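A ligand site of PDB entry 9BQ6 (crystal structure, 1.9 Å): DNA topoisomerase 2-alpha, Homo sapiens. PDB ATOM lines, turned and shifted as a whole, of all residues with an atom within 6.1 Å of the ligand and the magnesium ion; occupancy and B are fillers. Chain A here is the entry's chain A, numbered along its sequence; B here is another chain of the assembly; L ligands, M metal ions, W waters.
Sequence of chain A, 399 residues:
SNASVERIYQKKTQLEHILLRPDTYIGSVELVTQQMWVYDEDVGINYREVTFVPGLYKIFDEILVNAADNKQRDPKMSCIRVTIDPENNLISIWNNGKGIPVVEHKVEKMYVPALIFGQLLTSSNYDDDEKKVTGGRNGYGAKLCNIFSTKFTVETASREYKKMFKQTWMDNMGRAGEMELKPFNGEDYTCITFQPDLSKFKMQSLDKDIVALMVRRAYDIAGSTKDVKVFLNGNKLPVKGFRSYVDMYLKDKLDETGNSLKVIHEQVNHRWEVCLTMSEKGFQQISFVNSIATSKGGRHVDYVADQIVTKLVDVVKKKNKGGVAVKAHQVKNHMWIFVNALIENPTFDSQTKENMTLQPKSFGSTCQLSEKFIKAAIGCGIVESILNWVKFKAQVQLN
O5 of the ligand is in hydrogen-bond range of ND2 of Asn 125 (3.0 Å). N of Arg 137 lies within hydrogen-bond range of O2 of the ligand, at 2.9 Å. An oxygen (O7) of the ligand sits at hydrogen-bond distance from the backbone NH (N) of Ala 142, at 3.0 Å. NE2 of Gln 351 lies within hydrogen-bond range of O3 of the ligand, at 3.2 Å. NZ of Lys 353 lies within salt-bridge range of O2 of the ligand. N of Tyr 140 lies within hydrogen-bond range of O3 of the ligand, at 2.7 Å. NZ of Lys 143 is in salt-bridge range of O7 of the ligand, 2.6 Å away. N of Gly 141 lies within hydrogen-bond range of O3 of the ligand (2.9 Å). O12 of the ligand lies within hydrogen-bond range of OG of Ser 124 (2.8 Å). N of Gly 139 lies within hydrogen-bond range of O3 of the ligand, at 3.1 Å. OD1 of Asn 70 lies close to N5 of the ligand. N4 of the ligand sits at hydrogen-bond distance from OD1 of Asn 95, at 3.0 Å. N of Ser 124 is in hydrogen-bond range of O11 of the ligand, at 3.1 Å. The side-chain hydroxyl of Ser 123 is in hydrogen-bond range of an oxygen (O5) of the ligand, at 2.7 Å. An oxygen (O2) of the ligand is in hydrogen-bond range of the backbone NH (N) of Asn 138 (3.1 Å).
The side-chain hydroxyl (OG1) of Thr 156 is in hydrogen-bond range of the side-chain hydroxyl (OG1) of Thr 190 (2.7 Å). The backbone NH (N) of Asn 95 sits at hydrogen-bond distance from the backbone carbonyl oxygen (O) of Thr 190 (3.0 Å). ND2 of Asn 70 lies within hydrogen-bond range of O of Lys 98, 3.4 Å away. OD1 of Asn 70 is in hydrogen-bond range of NH1 of Arg 73 (3.0 Å). The side-chain carboxylate of Asp 69 sits at hydrogen-bond distance from the backbone NH of Gly 136 (3.1 Å). The side-chain amide nitrogen (ND2) of Asn 70 lies close to the side-chain amide nitrogen (ND2) of Asn 95 (3.4 Å). The backbone NH of Asn 125 lies within hydrogen-bond range of the side-chain hydroxyl of Ser 123, at 2.8 Å. The backbone carbonyl oxygen (O) of Gly 135 lies within hydrogen-bond range of the side-chain amino group (NZ) of Lys 353 (2.9 Å).
Residues that only touch the ligand: Glu 62 (3.6 Å), Arg 73 (3.95 Å), Ile 100 (3.6 Å), Ile 116 (3.2 Å), Phe 117 (3.6 Å), Thr 122 (3.7 Å), Gly 136 (3.5 Å), Thr 190 (3.7 Å) and Tyr 9 of chain B (3.5 Å). Hydrophobic or aromatic side chains that line the ligand: Ile 100, Ile 116, Phe 117, Tyr 140, Ala 142 and Tyr 9 of chain B. The nearest printed residue that does not touch the ligand is Ala 67 (4.1 Å).
One residue has an atom within 4 Å of the magnesium ion: Asn 66. The nearest printed residue that does not touch the magnesium ion is Glu 62 (4.1 Å).
The magnesium ion is bound by an oxygen (O1) of the ligand (2.0 Å), an oxygen (O4) of the ligand (2.1 Å), an oxygen (O6) of the ligand (2.1 Å), the side-chain amide oxygen of Asn 66 (2.1 Å), water W5 (2.2 Å) and water W8 (2.2 Å). The magnesium ion has six donor atoms within binding distance.
Water W8 lies within hydrogen-bond range of the side-chain carboxylate (OE1) of Glu 62 (2.5 Å) and the side-chain amide nitrogen (ND2) of Asn 66 (3.4 Å). Water W5 bridges OD2 of Asp 69 (3.1 Å) and N of Gly 136 (3.4 Å). Water W9 lies within hydrogen-bond range of OG1 of Thr 190 (2.6 Å), N5 of the ligand (2.8 Å), O of Lys 98 (2.8 Å) and ND2 of Asn 95 (3.1 Å). Water W6 bridges ND2 of Asn 66 (2.8 Å) and N3 of the ligand (2.9 Å). Water W7 lies within hydrogen-bond range of OH of Tyr 9 of chain B (2.7 Å), N6 of the ligand (2.9 Å) and NE of Arg 73 (3.4 Å). Water W4 lies within hydrogen-bond range of O of Ile 63, N4 of the ligand and N of Ala 67.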
ATOM      1  N   GLU A  62     -20.878 -16.646  23.869  1.00  0.00           N
ATOM      2  CA  GLU A  62     -20.997 -15.630  24.908  1.00  0.00           C
ATOM      3  C   GLU A  62     -21.123 -14.234  24.311  1.00  0.00           C
ATOM      4  O   GLU A  62     -21.935 -13.422  24.780  1.00  0.00           O
ATOM      5  CB  GLU A  62     -19.815 -15.725  25.865  1.00  0.00           C
ATOM      6  CG  GLU A  62     -19.761 -16.984  26.753  1.00  0.00           C
ATOM      7  CD  GLU A  62     -20.851 -17.048  27.822  1.00  0.00           C
ATOM      8  OE1 GLU A  62     -21.712 -16.126  27.882  1.00  0.00           O
ATOM      9  OE2 GLU A  62     -20.871 -18.012  28.620  1.00  0.00           O
ATOM     10  N   ILE A  63     -20.296 -13.922  23.301  1.00  0.00           N
ATOM     11  CA  ILE A  63     -20.290 -12.592  22.734  1.00  0.00           C
ATOM     12  C   ILE A  63     -21.538 -12.390  21.894  1.00  0.00           C
ATOM     13  O   ILE A  63     -22.107 -11.298  21.868  1.00  0.00           O
ATOM     14  CB  ILE A  63     -19.013 -12.379  21.895  1.00  0.00           C
ATOM     15  CG1 ILE A  63     -17.744 -12.651  22.707  1.00  0.00           C
ATOM     16  CG2 ILE A  63     -19.017 -10.982  21.310  1.00  0.00           C
ATOM     17  CD1 ILE A  63     -17.574 -11.837  23.962  1.00  0.00           C
ATOM     18  N   VAL A  65     -24.543 -13.842  22.330  1.00  0.00           N
ATOM     19  CA  VAL A  65     -25.716 -13.621  23.179  1.00  0.00           C
ATOM     20  C   VAL A  65     -25.664 -12.237  23.814  1.00  0.00           C
ATOM     21  O   VAL A  65     -26.697 -11.586  23.968  1.00  0.00           O
ATOM     22  CB  VAL A  65     -25.814 -14.705  24.259  1.00  0.00           C
ATOM     23  CG1 VAL A  65     -26.943 -14.365  25.254  1.00  0.00           C
ATOM     24  CG2 VAL A  65     -26.052 -16.069  23.649  1.00  0.00           C
ATOM     25  N   ASN A  66     -24.472 -11.755  24.167  1.00  0.00           N
ATOM     26  CA  ASN A  66     -24.348 -10.381  24.653  1.00  0.00           C
ATOM     27  C   ASN A  66     -24.926  -9.393  23.655  1.00  0.00           C
ATOM     28  O   ASN A  66     -25.547  -8.384  24.048  1.00  0.00           O
ATOM     29  CB  ASN A  66     -22.897 -10.050  24.924  1.00  0.00           C
ATOM     30  CG  ASN A  66     -22.409 -10.557  26.249  1.00  0.00           C
ATOM     31  OD1 ASN A  66     -23.173 -11.022  27.089  1.00  0.00           O
ATOM     32  ND2 ASN A  66     -21.084 -10.548  26.409  1.00  0.00           N
ATOM     33  N   ALA A  67     -24.662  -9.630  22.362  1.00  0.00           N
ATOM     34  CA  ALA A  67     -25.176  -8.742  21.336  1.00  0.00           C
ATOM     35  C   ALA A  67     -26.694  -8.793  21.304  1.00  0.00           C
ATOM     36  O   ALA A  67     -27.351  -7.757  21.189  1.00  0.00           O
ATOM     37  CB  ALA A  67     -24.609  -9.102  19.976  1.00  0.00           C
ATOM     38  N   ASP A  69     -28.649  -9.625  23.768  1.00  0.00           N
ATOM     39  CA  ASP A  69     -29.102  -8.980  24.997  1.00  0.00           C
ATOM     40  C   ASP A  69     -29.298  -7.483  24.812  1.00  0.00           C
ATOM     41  O   ASP A  69     -30.141  -6.885  25.486  1.00  0.00           O
ATOM     42  CB  ASP A  69     -28.070  -9.210  26.102  1.00  0.00           C
ATOM     43  CG  ASP A  69     -28.077 -10.625  26.625  1.00  0.00           C
ATOM     44  OD1 ASP A  69     -29.033 -11.378  26.325  1.00  0.00           O
ATOM     45  OD2 ASP A  69     -27.139 -10.985  27.363  1.00  0.00           O
ATOM     46  N   ASN A  70     -28.516  -6.845  23.943  1.00  0.00           N
ATOM     47  CA  ASN A  70     -28.606  -5.400  23.852  1.00  0.00           C
ATOM     48  C   ASN A  70     -29.935  -4.961  23.245  1.00  0.00           C
ATOM     49  O   ASN A  70     -30.341  -3.818  23.465  1.00  0.00           O
ATOM     50  CB  ASN A  70     -27.456  -4.819  23.032  1.00  0.00           C
ATOM     51  CG  ASN A  70     -27.248  -3.342  23.323  1.00  0.00           C
ATOM     52  OD1 ASN A  70     -26.991  -2.966  24.460  1.00  0.00           O
ATOM     53  ND2 ASN A  70     -27.397  -2.503  22.303  1.00  0.00           N
ATOM     54  N   ARG A  73     -32.070  -4.318  26.212  1.00  0.00           N
ATOM     55  CA  ARG A  73     -31.647  -3.055  26.806  1.00  0.00           C
ATOM     56  C   ARG A  73     -32.085  -1.855  25.972  1.00  0.00           C
ATOM     57  O   ARG A  73     -32.456  -0.818  26.516  1.00  0.00           O
ATOM     58  CB  ARG A  73     -30.117  -3.067  26.981  1.00  0.00           C
ATOM     59  CG  ARG A  73     -29.526  -1.731  27.414  1.00  0.00           C
ATOM     60  CD  ARG A  73     -28.062  -1.929  27.830  1.00  0.00           C
ATOM     61  NE  ARG A  73     -27.442  -0.631  28.112  1.00  0.00           N
ATOM     62  CZ  ARG A  73     -26.651   0.015  27.262  1.00  0.00           C
ATOM     63  NH1 ARG A  73     -26.360  -0.507  26.092  1.00  0.00           N
ATOM     64  NH2 ARG A  73     -26.151   1.196  27.601  1.00  0.00           N
ATOM     65  N   ASN A  95     -22.927  -4.796  16.967  1.00  0.00           N
ATOM     66  CA  ASN A  95     -24.349  -4.550  17.145  1.00  0.00           C
ATOM     67  C   ASN A  95     -24.555  -3.053  17.270  1.00  0.00           C
ATOM     68  O   ASN A  95     -23.637  -2.345  17.702  1.00  0.00           O
ATOM     69  CB  ASN A  95     -24.926  -5.228  18.390  1.00  0.00           C
ATOM     70  CG  ASN A  95     -24.366  -4.644  19.684  1.00  0.00           C
ATOM     71  OD1 ASN A  95     -23.402  -5.159  20.254  1.00  0.00           O
ATOM     72  ND2 ASN A  95     -24.949  -3.534  20.137  1.00  0.00           N
ATOM     73  N   LYS A  98     -27.819   1.319  21.843  1.00  0.00           N
ATOM     74  CA  LYS A  98     -27.050   2.100  22.798  1.00  0.00           C
ATOM     75  C   LYS A  98     -25.727   1.431  23.136  1.00  0.00           C
ATOM     76  O   LYS A  98     -25.669   0.232  23.438  1.00  0.00           O
ATOM     77  CB  LYS A  98     -27.889   2.284  24.064  1.00  0.00           C
ATOM     78  CG  LYS A  98     -27.520   3.442  24.954  1.00  0.00           C
ATOM     79  CD  LYS A  98     -28.575   3.599  26.050  1.00  0.00           C
ATOM     80  CE  LYS A  98     -28.379   4.884  26.819  1.00  0.00           C
ATOM     81  NZ  LYS A  98     -27.024   4.952  27.420  1.00  0.00           N
ATOM     82  N   GLY A  99     -24.652   2.221  23.086  1.00  0.00           N
ATOM     83  CA  GLY A  99     -23.345   1.758  23.481  1.00  0.00           C
ATOM     84  C   GLY A  99     -23.209   1.722  24.991  1.00  0.00           C
ATOM     85  O   GLY A  99     -24.089   2.118  25.746  1.00  0.00           O
ATOM     86  N   ILE A 100     -22.063   1.218  25.425  1.00  0.00           N
ATOM     87  CA  ILE A 100     -21.721   1.141  26.841  1.00  0.00           C
ATOM     88  C   ILE A 100     -21.304   2.547  27.261  1.00  0.00           C
ATOM     89  O   ILE A 100     -20.659   3.261  26.486  1.00  0.00           O
ATOM     90  CB  ILE A 100     -20.636   0.081  27.074  1.00  0.00           C
ATOM     91  CG1 ILE A 100     -21.209  -1.250  26.599  1.00  0.00           C
ATOM     92  CG2 ILE A 100     -20.250   0.010  28.514  1.00  0.00           C
ATOM     93  CD1 ILE A 100     -20.210  -2.359  26.434  1.00  0.00           C
ATOM     94  N   ILE A 116     -16.097  -3.943  32.654  1.00  0.00           N
ATOM     95  CA  ILE A 116     -17.001  -5.068  32.450  1.00  0.00           C
ATOM     96  C   ILE A 116     -16.498  -6.034  31.387  1.00  0.00           C
ATOM     97  O   ILE A 116     -17.092  -7.111  31.216  1.00  0.00           O
ATOM     98  CB  ILE A 116     -18.412  -4.589  32.081  1.00  0.00           C
ATOM     99  CG1 ILE A 116     -18.429  -3.940  30.700  1.00  0.00           C
ATOM    100  CG2 ILE A 116     -18.903  -3.605  33.146  1.00  0.00           C
ATOM    101  CD1 ILE A 116     -19.759  -3.273  30.334  1.00  0.00           C
ATOM    102  N   PHE A 117     -15.434  -5.697  30.658  1.00  0.00           N
ATOM    103  CA  PHE A 117     -14.799  -6.656  29.758  1.00  0.00           C
ATOM    104  C   PHE A 117     -13.464  -7.166  30.260  1.00  0.00           C
ATOM    105  O   PHE A 117     -12.992  -8.195  29.777  1.00  0.00           O
ATOM    106  CB  PHE A 117     -14.613  -6.036  28.349  1.00  0.00           C
ATOM    107  CG  PHE A 117     -15.898  -5.973  27.569  1.00  0.00           C
ATOM    108  CD1 PHE A 117     -16.316  -7.066  26.832  1.00  0.00           C
ATOM    109  CD2 PHE A 117     -16.700  -4.828  27.591  1.00  0.00           C
ATOM    110  CE1 PHE A 117     -17.512  -7.035  26.120  1.00  0.00           C
ATOM    111  CE2 PHE A 117     -17.900  -4.785  26.887  1.00  0.00           C
ATOM    112  CZ  PHE A 117     -18.308  -5.901  26.149  1.00  0.00           C
ATOM    113  N   THR A 122     -18.338  -8.903  36.747  1.00  0.00           N
ATOM    114  CA  THR A 122     -18.839  -7.562  36.473  1.00  0.00           C
ATOM    115  C   THR A 122     -20.019  -7.699  35.525  1.00  0.00           C
ATOM    116  O   THR A 122     -19.935  -8.435  34.526  1.00  0.00           O
ATOM    117  CB  THR A 122     -17.764  -6.682  35.841  1.00  0.00           C
ATOM    118  OG1 THR A 122     -17.211  -7.351  34.714  1.00  0.00           O
ATOM    119  CG2 THR A 122     -16.649  -6.360  36.847  1.00  0.00           C
ATOM    120  N   SER A 123     -21.113  -7.001  35.829  1.00  0.00           N
ATOM    121  CA  SER A 123     -22.358  -7.237  35.105  1.00  0.00           C
ATOM    122  C   SER A 123     -23.354  -6.117  35.423  1.00  0.00           C
ATOM    123  O   SER A 123     -23.265  -5.460  36.465  1.00  0.00           O
ATOM    124  CB  SER A 123     -22.959  -8.582  35.483  1.00  0.00           C
ATOM    125  OG  SER A 123     -24.211  -8.805  34.863  1.00  0.00           O
ATOM    126  N   SER A 124     -24.264  -5.879  34.491  1.00  0.00           N
ATOM    127  CA  SER A 124     -25.450  -5.070  34.764  1.00  0.00           C
ATOM    128  C   SER A 124     -26.634  -5.915  35.216  1.00  0.00           C
ATOM    129  O   SER A 124     -27.736  -5.375  35.369  1.00  0.00           O
ATOM    130  CB  SER A 124     -25.860  -4.284  33.501  1.00  0.00           C
ATOM    131  OG  SER A 124     -26.065  -5.170  32.409  1.00  0.00           O
ATOM    132  N   ASN A 125     -26.433  -7.227  35.389  1.00  0.00           N
ATOM    133  CA  ASN A 125     -27.523  -8.161  35.633  1.00  0.00           C
ATOM    134  C   ASN A 125     -27.547  -8.713  37.045  1.00  0.00           C
ATOM    135  O   ASN A 125     -28.096  -9.791  37.280  1.00  0.00           O
ATOM    136  CB  ASN A 125     -27.436  -9.316  34.631  1.00  0.00           C
ATOM    137  CG  ASN A 125     -27.803  -8.884  33.245  1.00  0.00           C
ATOM    138  OD1 ASN A 125     -28.943  -8.452  33.008  1.00  0.00           O
ATOM    139  ND2 ASN A 125     -26.873  -8.992  32.323  1.00  0.00           N
ATOM    140  N   GLY A 135     -30.220 -12.743  28.371  1.00  0.00           N
ATOM    141  CA  GLY A 135     -29.517 -13.990  28.649  1.00  0.00           C
ATOM    142  C   GLY A 135     -28.395 -13.871  29.658  1.00  0.00           C
ATOM    143  O   GLY A 135     -28.036 -14.861  30.287  1.00  0.00           O
ATOM    144  N   GLY A 136     -27.881 -12.659  29.852  1.00  0.00           N
ATOM    145  CA  GLY A 136     -26.773 -12.478  30.778  1.00  0.00           C
ATOM    146  C   GLY A 136     -27.256 -12.568  32.227  1.00  0.00           C
ATOM    147  O   GLY A 136     -28.276 -11.986  32.604  1.00  0.00           O
ATOM    148  N   ARG A 137     -26.503 -13.288  33.035  1.00  0.00           N
ATOM    149  CA  ARG A 137     -26.833 -13.444  34.435  1.00  0.00           C
ATOM    150  C   ARG A 137     -25.639 -13.319  35.367  1.00  0.00           C
ATOM    151  O   ARG A 137     -25.748 -12.764  36.449  1.00  0.00           O
ATOM    152  CB  ARG A 137     -27.487 -14.819  34.640  1.00  0.00           C
ATOM    153  CG  ARG A 137     -28.751 -15.079  33.776  1.00  0.00           C
ATOM    154  CD  ARG A 137     -29.938 -14.237  34.179  1.00  0.00           C
ATOM    155  NE  ARG A 137     -30.288 -14.518  35.568  1.00  0.00           N
ATOM    156  CZ  ARG A 137     -30.539 -13.631  36.522  1.00  0.00           C
ATOM    157  NH1 ARG A 137     -30.498 -12.340  36.251  1.00  0.00           N
ATOM    158  NH2 ARG A 137     -30.800 -14.061  37.748  1.00  0.00           N
ATOM    159  N   ASN A 138     -24.468 -13.803  34.963  1.00  0.00           N
ATOM    160  CA  ASN A 138     -23.429 -14.113  35.934  1.00  0.00           C
ATOM    161  C   ASN A 138     -22.243 -13.167  35.957  1.00  0.00           C
ATOM    162  O   ASN A 138     -21.501 -13.176  36.953  1.00  0.00           O
ATOM    163  CB  ASN A 138     -22.885 -15.529  35.697  1.00  0.00           C
ATOM    164  CG  ASN A 138     -23.945 -16.568  35.820  1.00  0.00           C
ATOM    165  OD1 ASN A 138     -24.825 -16.472  36.671  1.00  0.00           O
ATOM    166  ND2 ASN A 138     -23.872 -17.585  34.977  1.00  0.00           N
ATOM    167  N   GLY A 139     -22.023 -12.396  34.905  1.00  0.00           N
ATOM    168  CA  GLY A 139     -20.891 -11.500  34.873  1.00  0.00           C
ATOM    169  C   GLY A 139     -19.576 -12.144  34.491  1.00  0.00           C
ATOM    170  O   GLY A 139     -18.517 -11.609  34.852  1.00  0.00           O
ATOM    171  N   TYR A 140     -19.622 -13.251  33.747  1.00  0.00           N
ATOM    172  CA  TYR A 140     -18.431 -13.970  33.280  1.00  0.00           C
ATOM    173  C   TYR A 140     -18.204 -13.912  31.784  1.00  0.00           C
ATOM    174  O   TYR A 140     -17.053 -13.854  31.338  1.00  0.00           O
ATOM    175  CB  TYR A 140     -18.533 -15.455  33.667  1.00  0.00           C
ATOM    176  CG  TYR A 140     -17.933 -15.859  34.997  1.00  0.00           C
ATOM    177  CD1 TYR A 140     -16.559 -15.784  35.196  1.00  0.00           C
ATOM    178  CD2 TYR A 140     -18.726 -16.370  36.017  1.00  0.00           C
ATOM    179  CE1 TYR A 140     -15.998 -16.167  36.387  1.00  0.00           C
ATOM    180  CE2 TYR A 140     -18.159 -16.768  37.223  1.00  0.00           C
ATOM    181  CZ  TYR A 140     -16.799 -16.650  37.400  1.00  0.00           C
ATOM    182  OH  TYR A 140     -16.200 -17.030  38.588  1.00  0.00           O
ATOM    183  N   GLY A 141     -19.288 -14.049  31.023  1.00  0.00           N
ATOM    184  CA  GLY A 141     -19.198 -14.478  29.632  1.00  0.00           C
ATOM    185  C   GLY A 141     -18.158 -13.744  28.804  1.00  0.00           C
ATOM    186  O   GLY A 141     -17.350 -14.374  28.112  1.00  0.00           O
ATOM    187  N   ALA A 142     -18.215 -12.406  28.796  1.00  0.00           N
ATOM    188  CA  ALA A 142     -17.266 -11.668  27.976  1.00  0.00           C
ATOM    189  C   ALA A 142     -15.837 -11.847  28.458  1.00  0.00           C
ATOM    190  O   ALA A 142     -14.922 -11.937  27.641  1.00  0.00           O
ATOM    191  CB  ALA A 142     -17.628 -10.193  27.924  1.00  0.00           C
ATOM    192  N   LYS A 143     -15.627 -11.896  29.781  1.00  0.00           N
ATOM    193  CA  LYS A 143     -14.284 -12.086  30.287  1.00  0.00           C
ATOM    194  C   LYS A 143     -13.764 -13.475  29.907  1.00  0.00           C
ATOM    195  O   LYS A 143     -12.586 -13.635  29.616  1.00  0.00           O
ATOM    196  CB  LYS A 143     -14.234 -11.897  31.804  1.00  0.00           C
ATOM    197  CG  LYS A 143     -14.093 -10.418  32.288  1.00  0.00           C
ATOM    198  CD  LYS A 143     -15.367  -9.602  31.982  1.00  0.00           C
ATOM    199  CE  LYS A 143     -16.552 -10.074  32.829  1.00  0.00           C
ATOM    200  NZ  LYS A 143     -17.827  -9.305  32.601  1.00  0.00           N
ATOM    201  N   THR A 156     -16.715   0.583  21.678  1.00  0.00           N
ATOM    202  CA  THR A 156     -18.103   0.927  21.961  1.00  0.00           C
ATOM    203  C   THR A 156     -18.193   2.443  21.893  1.00  0.00           C
ATOM    204  O   THR A 156     -17.260   3.145  22.300  1.00  0.00           O
ATOM    205  CB  THR A 156     -18.562   0.384  23.317  1.00  0.00           C
ATOM    206  OG1 THR A 156     -19.984   0.551  23.444  1.00  0.00           O
ATOM    207  CG2 THR A 156     -17.868   1.075  24.477  1.00  0.00           C
ATOM    208  N   THR A 190     -21.490  -1.261  19.486  1.00  0.00           N
ATOM    209  CA  THR A 190     -20.453  -1.975  20.197  1.00  0.00           C
ATOM    210  C   THR A 190     -19.905  -3.016  19.240  1.00  0.00           C
ATOM    211  O   THR A 190     -20.665  -3.689  18.536  1.00  0.00           O
ATOM    212  CB  THR A 190     -21.006  -2.625  21.478  1.00  0.00           C
ATOM    213  OG1 THR A 190     -21.334  -1.607  22.416  1.00  0.00           O
ATOM    214  CG2 THR A 190     -19.983  -3.580  22.091  1.00  0.00           C
ATOM    215  N   ILE A 192     -17.020  -6.221  19.246  1.00  0.00           N
ATOM    216  CA  ILE A 192     -16.028  -7.065  19.900  1.00  0.00           C
ATOM    217  C   ILE A 192     -15.323  -7.869  18.812  1.00  0.00           C
ATOM    218  O   ILE A 192     -15.970  -8.639  18.081  1.00  0.00           O
ATOM    219  CB  ILE A 192     -16.674  -7.998  20.932  1.00  0.00           C
ATOM    220  CG1 ILE A 192     -17.661  -7.262  21.836  1.00  0.00           C
ATOM    221  CG2 ILE A 192     -15.583  -8.711  21.738  1.00  0.00           C
ATOM    222  CD1 ILE A 192     -17.092  -6.080  22.576  1.00  0.00           C
ATOM    223  N   GLN A 351     -22.432 -22.185  33.860  1.00  0.00           N
ATOM    224  CA  GLN A 351     -22.214 -20.994  33.054  1.00  0.00           C
ATOM    225  C   GLN A 351     -22.525 -21.242  31.604  1.00  0.00           C
ATOM    226  O   GLN A 351     -22.885 -20.300  30.885  1.00  0.00           O
ATOM    227  CB  GLN A 351     -20.739 -20.543  33.190  1.00  0.00           C
ATOM    228  CG  GLN A 351     -20.371 -19.408  32.233  1.00  0.00           C
ATOM    229  CD  GLN A 351     -21.049 -18.067  32.563  1.00  0.00           C
ATOM    230  OE1 GLN A 351     -21.369 -17.804  33.729  1.00  0.00           O
ATOM    231  NE2 GLN A 351     -21.276 -17.244  31.564  1.00  0.00           N
ATOM    232  N   LYS A 353     -25.006 -22.693  30.361  1.00  0.00           N
ATOM    233  CA  LYS A 353     -26.441 -22.410  30.186  1.00  0.00           C
ATOM    234  C   LYS A 353     -27.097 -23.336  29.172  1.00  0.00           C
ATOM    235  O   LYS A 353     -27.949 -22.920  28.391  1.00  0.00           O
ATOM    236  CB  LYS A 353     -26.663 -20.930  29.804  1.00  0.00           C
ATOM    237  CG  LYS A 353     -26.119 -19.893  30.807  1.00  0.00           C
ATOM    238  CD  LYS A 353     -26.311 -18.473  30.283  1.00  0.00           C
ATOM    239  CE  LYS A 353     -25.522 -17.425  31.053  1.00  0.00           C
ATOM    240  NZ  LYS A 353     -25.458 -16.129  30.283  1.00  0.00           N
ATOM    241  N   TYR B   9     -23.821  -0.919  36.754  1.00  0.00           N
ATOM    242  CA  TYR B   9     -22.694  -1.805  36.541  1.00  0.00           C
ATOM    243  C   TYR B   9     -21.996  -2.089  37.870  1.00  0.00           C
ATOM    244  O   TYR B   9     -21.449  -1.178  38.503  1.00  0.00           O
ATOM    245  CB  TYR B   9     -21.736  -1.203  35.527  1.00  0.00           C
ATOM    246  CG  TYR B   9     -22.367  -0.960  34.184  1.00  0.00           C
ATOM    247  CD1 TYR B   9     -22.487  -1.989  33.246  1.00  0.00           C
ATOM    248  CD2 TYR B   9     -22.886   0.294  33.850  1.00  0.00           C
ATOM    249  CE1 TYR B   9     -23.071  -1.763  32.010  1.00  0.00           C
ATOM    250  CE2 TYR B   9     -23.480   0.520  32.625  1.00  0.00           C
ATOM    251  CZ  TYR B   9     -23.561  -0.511  31.705  1.00  0.00           C
ATOM    252  OH  TYR B   9     -24.163  -0.279  30.481  1.00  0.00           O
HETATM  253  P1  LIG L   1     -23.085 -13.805  31.680  1.00  0.00           P
HETATM  254  O1  LIG L   1     -22.881 -13.654  30.203  1.00  0.00           O
HETATM  255  O2  LIG L   1     -24.246 -14.786  32.073  1.00  0.00           O
HETATM  256  O3  LIG L   1     -21.787 -14.233  32.398  1.00  0.00           O
HETATM  257  P2  LIG L   1     -23.318 -10.936  31.538  1.00  0.00           P
HETATM  258  O4  LIG L   1     -23.738 -10.889  30.123  1.00  0.00           O
HETATM  259  O5  LIG L   1     -23.964  -9.793  32.349  1.00  0.00           O
HETATM  260  N1  LIG L   1     -23.662 -12.343  32.325  1.00  0.00           N
HETATM  261  P3  LIG L   1     -20.763 -10.508  30.403  1.00  0.00           P
HETATM  262  O6  LIG L   1     -21.124 -11.278  29.186  1.00  0.00           O
HETATM  263  O7  LIG L   1     -19.355 -10.710  30.974  1.00  0.00           O
HETATM  264  O8  LIG L   1     -21.731 -10.712  31.623  1.00  0.00           O
HETATM  265  O9  LIG L   1     -20.965  -8.996  29.961  1.00  0.00           O
HETATM  266  C1  LIG L   1     -20.699  -8.019  30.955  1.00  0.00           C
HETATM  267  C2  LIG L   1     -21.602  -6.809  30.806  1.00  0.00           C
HETATM  268  O10 LIG L   1     -21.179  -6.044  29.658  1.00  0.00           O
HETATM  269  C3  LIG L   1     -23.061  -7.139  30.558  1.00  0.00           C
HETATM  270  O11 LIG L   1     -23.732  -7.296  31.806  1.00  0.00           O
HETATM  271  C4  LIG L   1     -23.547  -5.921  29.786  1.00  0.00           C
HETATM  272  O12 LIG L   1     -23.888  -4.904  30.721  1.00  0.00           O
HETATM  273  C5  LIG L   1     -22.290  -5.446  29.051  1.00  0.00           C
HETATM  274  N2  LIG L   1     -22.252  -5.794  27.630  1.00  0.00           N
HETATM  275  C6  LIG L   1     -21.621  -6.867  27.065  1.00  0.00           C
HETATM  276  N3  LIG L   1     -21.750  -6.925  25.761  1.00  0.00           N
HETATM  277  C7  LIG L   1     -22.514  -5.807  25.461  1.00  0.00           C
HETATM  278  C8  LIG L   1     -22.995  -5.286  24.242  1.00  0.00           C
HETATM  279  N4  LIG L   1     -22.776  -5.861  23.060  1.00  0.00           N
HETATM  280  N5  LIG L   1     -23.723  -4.144  24.289  1.00  0.00           N
HETATM  281  C9  LIG L   1     -23.942  -3.569  25.471  1.00  0.00           C
HETATM  282  N6  LIG L   1     -23.537  -3.959  26.675  1.00  0.00           N
HETATM  283  C10 LIG L   1     -22.825  -5.098  26.602  1.00  0.00           C
HETATM  284 MG    MG M   1     -22.920 -12.282  28.800  1.00  0.00          MG
HETATM  285  O   HOH W   1     -26.620  -5.032  26.748  1.00  0.00           O
HETATM  286  O   HOH W   2     -25.045  -7.304  26.504  1.00  0.00           O
HETATM  287  O   HOH W   3     -25.423  -9.257  28.573  1.00  0.00           O
HETATM  288  O   HOH W   4     -21.436  -8.469  21.963  1.00  0.00           O
HETATM  289  O   HOH W   5     -24.884 -12.946  28.188  1.00  0.00           O
HETATM  290  O   HOH W   6     -19.967  -8.789  24.519  1.00  0.00           O
HETATM  291  O   HOH W   7     -24.617  -2.459  28.870  1.00  0.00           O
HETATM  292  O   HOH W   8     -21.972 -13.661  27.426  1.00  0.00           O
HETATM  293  O   HOH W   9     -23.942  -1.878  22.617  1.00  0.00           O
